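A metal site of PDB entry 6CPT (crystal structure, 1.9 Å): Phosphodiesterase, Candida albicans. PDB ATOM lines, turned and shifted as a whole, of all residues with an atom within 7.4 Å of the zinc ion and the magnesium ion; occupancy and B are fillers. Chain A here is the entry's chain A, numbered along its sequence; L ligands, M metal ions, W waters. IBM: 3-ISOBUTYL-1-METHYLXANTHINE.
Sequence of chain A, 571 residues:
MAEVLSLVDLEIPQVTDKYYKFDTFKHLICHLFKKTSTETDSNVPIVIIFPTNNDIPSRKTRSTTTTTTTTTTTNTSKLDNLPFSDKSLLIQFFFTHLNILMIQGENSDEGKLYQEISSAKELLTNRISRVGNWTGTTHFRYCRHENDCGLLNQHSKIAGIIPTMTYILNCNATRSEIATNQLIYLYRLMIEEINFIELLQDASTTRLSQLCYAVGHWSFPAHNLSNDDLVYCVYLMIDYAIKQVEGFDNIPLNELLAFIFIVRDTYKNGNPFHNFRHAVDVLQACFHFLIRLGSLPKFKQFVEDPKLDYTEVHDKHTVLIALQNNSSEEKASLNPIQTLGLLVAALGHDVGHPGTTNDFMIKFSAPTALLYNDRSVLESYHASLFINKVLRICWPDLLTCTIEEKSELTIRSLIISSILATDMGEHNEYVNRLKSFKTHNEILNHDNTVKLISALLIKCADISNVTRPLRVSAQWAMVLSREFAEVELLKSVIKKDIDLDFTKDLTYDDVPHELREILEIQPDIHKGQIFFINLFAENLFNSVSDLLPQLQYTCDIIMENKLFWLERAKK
The zinc ion is bound by water W1 (2.0 Å), OD1 of Asp 462 (2.1 Å), OD2 of Asp 350 (2.2 Å), water W2 (2.2 Å), NE2 of His 349 (2.3 Å) and NE2 of His 278 (2.4 Å).
One residue has an atom within 4 Å of the magnesium ion: Asp 350.
The nearest printed residue that does not touch the magnesium ion is His 382 (4.04 Å).
Water W5 lies within hydrogen-bond range of OE2 of Glu 379 and O of Thr 422.
Water W3 bridges the side-chain hydroxyl (OG1) of Thr 422 (2.7 Å) and the backbone carbonyl oxygen (O) of His 349 (2.8 Å).
Water W6 lies within hydrogen-bond range of NE2 of His 382 (2.8 Å) and OE2 of Glu 379 (3.3 Å).
Of the 23 residues printed, 4 come within 4 Å of the zinc ion.
The magnesium ion is bound by water W3 (2.0 Å), water W1 (2.0 Å), water W6 (2.1 Å), OD1 of Asp 350 (2.1 Å), water W4 (2.1 Å) and water W5 (2.2 Å).
N of Asp 350 is in hydrogen-bond range of OH of Tyr 267 (3.3 Å).
ND1 of His 349 sits at hydrogen-bond distance from O of Ala 346, 2.7 Å away.
OD1 of Asp 350 lies close to NE2 of His 382, at 3.4 Å.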
ATOM      1  N   TYR A 267      19.769 -38.200   9.486  1.00  0.00           N
ATOM      2  CA  TYR A 267      21.213 -38.010   9.314  1.00  0.00           C
ATOM      3  C   TYR A 267      21.932 -39.341   9.400  1.00  0.00           C
ATOM      4  O   TYR A 267      21.502 -40.235  10.130  1.00  0.00           O
ATOM      5  CB  TYR A 267      21.757 -37.001  10.323  1.00  0.00           C
ATOM      6  CG  TYR A 267      21.413 -35.567   9.965  1.00  0.00           C
ATOM      7  CD1 TYR A 267      20.249 -34.955  10.441  1.00  0.00           C
ATOM      8  CD2 TYR A 267      22.236 -34.834   9.124  1.00  0.00           C
ATOM      9  CE1 TYR A 267      19.935 -33.650  10.091  1.00  0.00           C
ATOM     10  CE2 TYR A 267      21.922 -33.529   8.774  1.00  0.00           C
ATOM     11  CZ  TYR A 267      20.781 -32.945   9.259  1.00  0.00           C
ATOM     12  OH  TYR A 267      20.496 -31.640   8.903  1.00  0.00           O
ATOM     13  N   PHE A 273      31.698 -36.049   9.040  1.00  0.00           N
ATOM     14  CA  PHE A 273      31.386 -34.629   9.153  1.00  0.00           C
ATOM     15  C   PHE A 273      29.900 -34.303   9.006  1.00  0.00           C
ATOM     16  O   PHE A 273      29.316 -33.713   9.904  1.00  0.00           O
ATOM     17  CB  PHE A 273      32.181 -33.844   8.123  1.00  0.00           C
ATOM     18  CG  PHE A 273      32.027 -32.353   8.240  1.00  0.00           C
ATOM     19  CD1 PHE A 273      32.958 -31.599   8.943  1.00  0.00           C
ATOM     20  CD2 PHE A 273      30.946 -31.712   7.659  1.00  0.00           C
ATOM     21  CE1 PHE A 273      32.819 -30.221   9.042  1.00  0.00           C
ATOM     22  CE2 PHE A 273      30.799 -30.341   7.766  1.00  0.00           C
ATOM     23  CZ  PHE A 273      31.734 -29.590   8.461  1.00  0.00           C
ATOM     24  N   HIS A 274      29.311 -34.665   7.868  1.00  0.00           N
ATOM     25  CA  HIS A 274      27.921 -34.288   7.572  1.00  0.00           C
ATOM     26  C   HIS A 274      26.904 -35.206   8.263  1.00  0.00           C
ATOM     27  O   HIS A 274      26.173 -35.953   7.620  1.00  0.00           O
ATOM     28  CB  HIS A 274      27.676 -34.266   6.063  1.00  0.00           C
ATOM     29  CG  HIS A 274      28.421 -33.186   5.364  1.00  0.00           C
ATOM     30  ND1 HIS A 274      29.599 -33.401   4.687  1.00  0.00           N
ATOM     31  CD2 HIS A 274      28.168 -31.854   5.261  1.00  0.00           C
ATOM     32  CE1 HIS A 274      30.036 -32.249   4.188  1.00  0.00           C
ATOM     33  NE2 HIS A 274      29.186 -31.301   4.530  1.00  0.00           N
ATOM     34  N   HIS A 278      26.920 -32.127  13.051  1.00  0.00           N
ATOM     35  CA  HIS A 278      27.092 -30.946  12.189  1.00  0.00           C
ATOM     36  C   HIS A 278      25.817 -30.119  12.076  1.00  0.00           C
ATOM     37  O   HIS A 278      25.861 -28.894  12.149  1.00  0.00           O
ATOM     38  CB  HIS A 278      27.591 -31.346  10.798  1.00  0.00           C
ATOM     39  CG  HIS A 278      27.609 -30.223   9.823  1.00  0.00           C
ATOM     40  ND1 HIS A 278      28.450 -29.135   9.941  1.00  0.00           N
ATOM     41  CD2 HIS A 278      26.875 -29.999   8.705  1.00  0.00           C
ATOM     42  CE1 HIS A 278      28.247 -28.306   8.950  1.00  0.00           C
ATOM     43  NE2 HIS A 278      27.299 -28.802   8.173  1.00  0.00           N
ATOM     44  N   ALA A 279      24.674 -30.792  11.907  1.00  0.00           N
ATOM     45  CA  ALA A 279      23.362 -30.107  11.872  1.00  0.00           C
ATOM     46  C   ALA A 279      23.128 -29.248  13.112  1.00  0.00           C
ATOM     47  O   ALA A 279      22.704 -28.088  13.014  1.00  0.00           O
ATOM     48  CB  ALA A 279      22.239 -31.127  11.719  1.00  0.00           C
ATOM     49  N   VAL A 282      25.565 -26.252  13.273  1.00  0.00           N
ATOM     50  CA  VAL A 282      25.103 -25.184  12.381  1.00  0.00           C
ATOM     51  C   VAL A 282      23.899 -24.451  13.003  1.00  0.00           C
ATOM     52  O   VAL A 282      23.828 -23.213  12.978  1.00  0.00           O
ATOM     53  CB  VAL A 282      24.771 -25.711  10.965  1.00  0.00           C
ATOM     54  CG1 VAL A 282      24.139 -24.622  10.108  1.00  0.00           C
ATOM     55  CG2 VAL A 282      26.039 -26.234  10.310  1.00  0.00           C
ATOM     56  N   ALA A 346      18.348 -24.503   9.508  1.00  0.00           N
ATOM     57  CA  ALA A 346      19.695 -24.923   9.899  1.00  0.00           C
ATOM     58  C   ALA A 346      19.703 -26.364  10.390  1.00  0.00           C
ATOM     59  O   ALA A 346      20.571 -27.140  10.010  1.00  0.00           O
ATOM     60  CB  ALA A 346      20.260 -24.002  10.982  1.00  0.00           C
ATOM     61  N   HIS A 349      19.275 -28.645   7.209  1.00  0.00           N
ATOM     62  CA  HIS A 349      19.921 -28.204   5.969  1.00  0.00           C
ATOM     63  C   HIS A 349      20.807 -29.261   5.294  1.00  0.00           C
ATOM     64  O   HIS A 349      21.130 -29.115   4.110  1.00  0.00           O
ATOM     65  CB  HIS A 349      20.753 -26.944   6.213  1.00  0.00           C
ATOM     66  CG  HIS A 349      22.125 -27.237   6.716  1.00  0.00           C
ATOM     67  ND1 HIS A 349      22.379 -27.541   8.033  1.00  0.00           N
ATOM     68  CD2 HIS A 349      23.313 -27.304   6.074  1.00  0.00           C
ATOM     69  CE1 HIS A 349      23.661 -27.793   8.179  1.00  0.00           C
ATOM     70  NE2 HIS A 349      24.252 -27.658   7.004  1.00  0.00           N
ATOM     71  N   ASP A 350      21.193 -30.313   6.014  1.00  0.00           N
ATOM     72  CA  ASP A 350      21.947 -31.414   5.416  1.00  0.00           C
ATOM     73  C   ASP A 350      21.265 -32.777   5.559  1.00  0.00           C
ATOM     74  O   ASP A 350      21.930 -33.802   5.464  1.00  0.00           O
ATOM     75  CB  ASP A 350      23.356 -31.499   6.050  1.00  0.00           C
ATOM     76  CG  ASP A 350      24.387 -30.630   5.334  1.00  0.00           C
ATOM     77  OD1 ASP A 350      24.230 -30.288   4.149  1.00  0.00           O
ATOM     78  OD2 ASP A 350      25.408 -30.360   5.978  1.00  0.00           O
ATOM     79  N   VAL A 351      19.946 -32.807   5.786  1.00  0.00           N
ATOM     80  CA  VAL A 351      19.263 -34.088   6.038  1.00  0.00           C
ATOM     81  C   VAL A 351      19.541 -35.104   4.918  1.00  0.00           C
ATOM     82  O   VAL A 351      19.463 -34.780   3.739  1.00  0.00           O
ATOM     83  CB  VAL A 351      17.723 -33.966   6.218  1.00  0.00           C
ATOM     84  CG1 VAL A 351      17.376 -33.141   7.459  1.00  0.00           C
ATOM     85  CG2 VAL A 351      17.058 -33.423   4.966  1.00  0.00           C
ATOM     86  N   HIS A 353      22.292 -36.443   4.067  1.00  0.00           N
ATOM     87  CA  HIS A 353      23.585 -36.262   3.406  1.00  0.00           C
ATOM     88  C   HIS A 353      24.318 -37.604   3.395  1.00  0.00           C
ATOM     89  O   HIS A 353      24.457 -38.225   4.444  1.00  0.00           O
ATOM     90  CB  HIS A 353      24.404 -35.180   4.128  1.00  0.00           C
ATOM     91  CG  HIS A 353      25.556 -34.647   3.340  1.00  0.00           C
ATOM     92  ND1 HIS A 353      26.615 -35.418   2.943  1.00  0.00           N
ATOM     93  CD2 HIS A 353      25.827 -33.389   2.891  1.00  0.00           C
ATOM     94  CE1 HIS A 353      27.492 -34.682   2.278  1.00  0.00           C
ATOM     95  NE2 HIS A 353      27.040 -33.445   2.238  1.00  0.00           N
ATOM     96  N   ASN A 358      28.943 -32.370  -4.006  1.00  0.00           N
ATOM     97  CA  ASN A 358      28.305 -32.160  -5.302  1.00  0.00           C
ATOM     98  C   ASN A 358      29.233 -32.550  -6.456  1.00  0.00           C
ATOM     99  O   ASN A 358      28.789 -33.187  -7.403  1.00  0.00           O
ATOM    100  CB  ASN A 358      27.835 -30.712  -5.474  1.00  0.00           C
ATOM    101  CG  ASN A 358      26.547 -30.432  -4.738  1.00  0.00           C
ATOM    102  OD1 ASN A 358      25.787 -31.340  -4.424  1.00  0.00           O
ATOM    103  ND2 ASN A 358      26.301 -29.162  -4.445  1.00  0.00           N
ATOM    104  N   LEU A 378      22.994 -32.001  -3.928  1.00  0.00           N
ATOM    105  CA  LEU A 378      22.741 -32.448  -2.567  1.00  0.00           C
ATOM    106  C   LEU A 378      21.759 -31.533  -1.837  1.00  0.00           C
ATOM    107  O   LEU A 378      20.890 -32.004  -1.136  1.00  0.00           O
ATOM    108  CB  LEU A 378      24.032 -32.596  -1.757  1.00  0.00           C
ATOM    109  CG  LEU A 378      24.929 -33.750  -2.204  1.00  0.00           C
ATOM    110  CD1 LEU A 378      26.225 -33.761  -1.395  1.00  0.00           C
ATOM    111  CD2 LEU A 378      24.223 -35.096  -2.093  1.00  0.00           C
ATOM    112  N   GLU A 379      21.889 -30.231  -2.047  1.00  0.00           N
ATOM    113  CA  GLU A 379      21.023 -29.275  -1.356  1.00  0.00           C
ATOM    114  C   GLU A 379      19.570 -29.365  -1.809  1.00  0.00           C
ATOM    115  O   GLU A 379      18.667 -29.177  -1.016  1.00  0.00           O
ATOM    116  CB  GLU A 379      21.551 -27.848  -1.538  1.00  0.00           C
ATOM    117  CG  GLU A 379      22.925 -27.623  -0.931  1.00  0.00           C
ATOM    118  CD  GLU A 379      24.059 -28.134  -1.803  1.00  0.00           C
ATOM    119  OE1 GLU A 379      23.865 -28.409  -3.015  1.00  0.00           O
ATOM    120  OE2 GLU A 379      25.172 -28.257  -1.268  1.00  0.00           O
ATOM    121  N   HIS A 382      18.396 -32.287   0.110  1.00  0.00           N
ATOM    122  CA  HIS A 382      18.132 -31.971   1.524  1.00  0.00           C
ATOM    123  C   HIS A 382      16.814 -31.227   1.686  1.00  0.00           C
ATOM    124  O   HIS A 382      16.037 -31.537   2.579  1.00  0.00           O
ATOM    125  CB  HIS A 382      19.240 -31.125   2.178  1.00  0.00           C
ATOM    126  CG  HIS A 382      20.606 -31.705   2.022  1.00  0.00           C
ATOM    127  ND1 HIS A 382      20.869 -33.048   2.158  1.00  0.00           N
ATOM    128  CD2 HIS A 382      21.784 -31.119   1.706  1.00  0.00           C
ATOM    129  CE1 HIS A 382      22.151 -33.272   1.922  1.00  0.00           C
ATOM    130  NE2 HIS A 382      22.731 -32.115   1.654  1.00  0.00           N
ATOM    131  N   ILE A 419      18.009 -23.410   2.707  1.00  0.00           N
ATOM    132  CA  ILE A 419      18.728 -24.654   2.491  1.00  0.00           C
ATOM    133  C   ILE A 419      19.471 -24.638   1.155  1.00  0.00           C
ATOM    134  O   ILE A 419      20.638 -25.033   1.078  1.00  0.00           O
ATOM    135  CB  ILE A 419      17.794 -25.874   2.607  1.00  0.00           C
ATOM    136  CG1 ILE A 419      17.331 -26.027   4.058  1.00  0.00           C
ATOM    137  CG2 ILE A 419      18.511 -27.133   2.153  1.00  0.00           C
ATOM    138  CD1 ILE A 419      16.333 -27.153   4.289  1.00  0.00           C
ATOM    139  N   THR A 422      22.942 -22.931   0.847  1.00  0.00           N
ATOM    140  CA  THR A 422      24.178 -23.546   1.382  1.00  0.00           C
ATOM    141  C   THR A 422      25.047 -24.238   0.338  1.00  0.00           C
ATOM    142  O   THR A 422      26.111 -24.741   0.664  1.00  0.00           O
ATOM    143  CB  THR A 422      23.892 -24.550   2.522  1.00  0.00           C
ATOM    144  OG1 THR A 422      23.098 -25.649   2.025  1.00  0.00           O
ATOM    145  CG2 THR A 422      23.152 -23.868   3.647  1.00  0.00           C
ATOM    146  N   ASP A 423      24.582 -24.290  -0.910  1.00  0.00           N
ATOM    147  CA  ASP A 423      25.391 -24.814  -1.990  1.00  0.00           C
ATOM    148  C   ASP A 423      26.595 -23.903  -2.251  1.00  0.00           C
ATOM    149  O   ASP A 423      26.425 -22.797  -2.733  1.00  0.00           O
ATOM    150  CB  ASP A 423      24.556 -24.936  -3.263  1.00  0.00           C
ATOM    151  CG  ASP A 423      25.353 -25.504  -4.435  1.00  0.00           C
ATOM    152  OD1 ASP A 423      26.481 -25.995  -4.231  1.00  0.00           O
ATOM    153  OD2 ASP A 423      24.834 -25.476  -5.570  1.00  0.00           O
ATOM    154  N   MET A 424      27.794 -24.391  -1.931  1.00  0.00           N
ATOM    155  CA  MET A 424      29.022 -23.601  -2.119  1.00  0.00           C
ATOM    156  C   MET A 424      29.344 -23.291  -3.568  1.00  0.00           C
ATOM    157  O   MET A 424      30.096 -22.357  -3.859  1.00  0.00           O
ATOM    158  CB  MET A 424      30.217 -24.310  -1.461  1.00  0.00           C
ATOM    159  CG  MET A 424      30.220 -24.265   0.062  1.00  0.00           C
ATOM    160  SD  MET A 424      30.318 -22.584   0.714  1.00  0.00           S
ATOM    161  CE  MET A 424      31.984 -22.153   0.246  1.00  0.00           C
ATOM    162  N   ILE A 458      22.639 -18.523   7.242  1.00  0.00           N
ATOM    163  CA  ILE A 458      22.759 -19.977   7.191  1.00  0.00           C
ATOM    164  C   ILE A 458      24.077 -20.361   6.491  1.00  0.00           C
ATOM    165  O   ILE A 458      24.724 -21.316   6.884  1.00  0.00           O
ATOM    166  CB  ILE A 458      21.499 -20.648   6.563  1.00  0.00           C
ATOM    167  CG1 ILE A 458      21.424 -22.130   6.955  1.00  0.00           C
ATOM    168  CG2 ILE A 458      21.463 -20.479   5.056  1.00  0.00           C
ATOM    169  CD1 ILE A 458      20.163 -22.823   6.479  1.00  0.00           C
ATOM    170  N   ALA A 461      26.720 -19.856   9.136  1.00  0.00           N
ATOM    171  CA  ALA A 461      26.602 -20.930  10.133  1.00  0.00           C
ATOM    172  C   ALA A 461      27.145 -22.238   9.598  1.00  0.00           C
ATOM    173  O   ALA A 461      27.856 -22.971  10.305  1.00  0.00           O
ATOM    174  CB  ALA A 461      25.151 -21.079  10.566  1.00  0.00           C
ATOM    175  N   ASP A 462      26.858 -22.526   8.333  1.00  0.00           N
ATOM    176  CA  ASP A 462      27.265 -23.780   7.712  1.00  0.00           C
ATOM    177  C   ASP A 462      28.783 -23.940   7.637  1.00  0.00           C
ATOM    178  O   ASP A 462      29.304 -25.033   7.824  1.00  0.00           O
ATOM    179  CB  ASP A 462      26.664 -23.909   6.318  1.00  0.00           C
ATOM    180  CG  ASP A 462      26.766 -25.305   5.744  1.00  0.00           C
ATOM    181  OD1 ASP A 462      26.806 -26.270   6.528  1.00  0.00           O
ATOM    182  OD2 ASP A 462      26.811 -25.424   4.513  1.00  0.00           O
ATOM    183  N   ILE A 463      29.500 -22.841   7.398  1.00  0.00           N
ATOM    184  CA  ILE A 463      30.959 -22.894   7.329  1.00  0.00           C
ATOM    185  C   ILE A 463      31.607 -22.269   8.573  1.00  0.00           C
ATOM    186  O   ILE A 463      32.756 -21.825   8.522  1.00  0.00           O
ATOM    187  CB  ILE A 463      31.518 -22.277   6.021  1.00  0.00           C
ATOM    188  CG1 ILE A 463      31.248 -20.766   5.953  1.00  0.00           C
ATOM    189  CG2 ILE A 463      30.906 -22.966   4.806  1.00  0.00           C
ATOM    190  CD1 ILE A 463      32.110 -20.058   4.937  1.00  0.00           C
HETATM  191  N9  IBM L   1      33.058 -26.228   4.804  1.00  0.00           N
HETATM  192  C8  IBM L   1      33.170 -25.926   6.127  1.00  0.00           C
HETATM  193  N7  IBM L   1      34.464 -26.006   6.532  1.00  0.00           N
HETATM  194  C5  IBM L   1      35.202 -26.375   5.460  1.00  0.00           C
HETATM  195  C4  IBM L   1      34.274 -26.518   4.328  1.00  0.00           C
HETATM  196  N3  IBM L   1      34.721 -26.887   3.114  1.00  0.00           N
HETATM  197  C2  IBM L   1      36.101 -27.134   2.908  1.00  0.00           C
HETATM  198  N1  IBM L   1      37.064 -27.010   3.946  1.00  0.00           N
HETATM  199  C6  IBM L   1      36.646 -26.635   5.248  1.00  0.00           C
HETATM  200  O6  IBM L   1      37.448 -26.510   6.210  1.00  0.00           O
HETATM  201  O2  IBM L   1      36.490 -27.468   1.757  1.00  0.00           O
HETATM  202  C10 IBM L   1      38.479 -27.286   3.660  1.00  0.00           C
HETATM  203  C11 IBM L   1      33.763 -26.997   2.004  1.00  0.00           C
HETATM  204  C12 IBM L   1      33.282 -28.427   1.758  1.00  0.00           C
HETATM  205  C13 IBM L   1      31.777 -28.541   1.943  1.00  0.00           C
HETATM  206  C14 IBM L   1      33.676 -28.896   0.359  1.00  0.00           C
HETATM  207 ZN    ZN M   1      26.263 -28.306   6.117  1.00  0.00          ZN
HETATM  208 MG    MG M   2      25.189 -29.098   2.728  1.00  0.00          MG
HETATM  209  O   HOH W   1      25.801 -27.828   4.187  1.00  0.00           O
HETATM  210  O   HOH W   2      28.267 -28.881   5.325  1.00  0.00           O
HETATM  211  O   HOH W   3      23.344 -28.289   2.609  1.00  0.00           O
HETATM  212  O   HOH W   4      27.160 -29.880   2.663  1.00  0.00           O
HETATM  213  O   HOH W   5      25.850 -27.600   1.277  1.00  0.00           O
HETATM  214  O   HOH W   6      24.935 -30.431   1.144  1.00  0.00           O
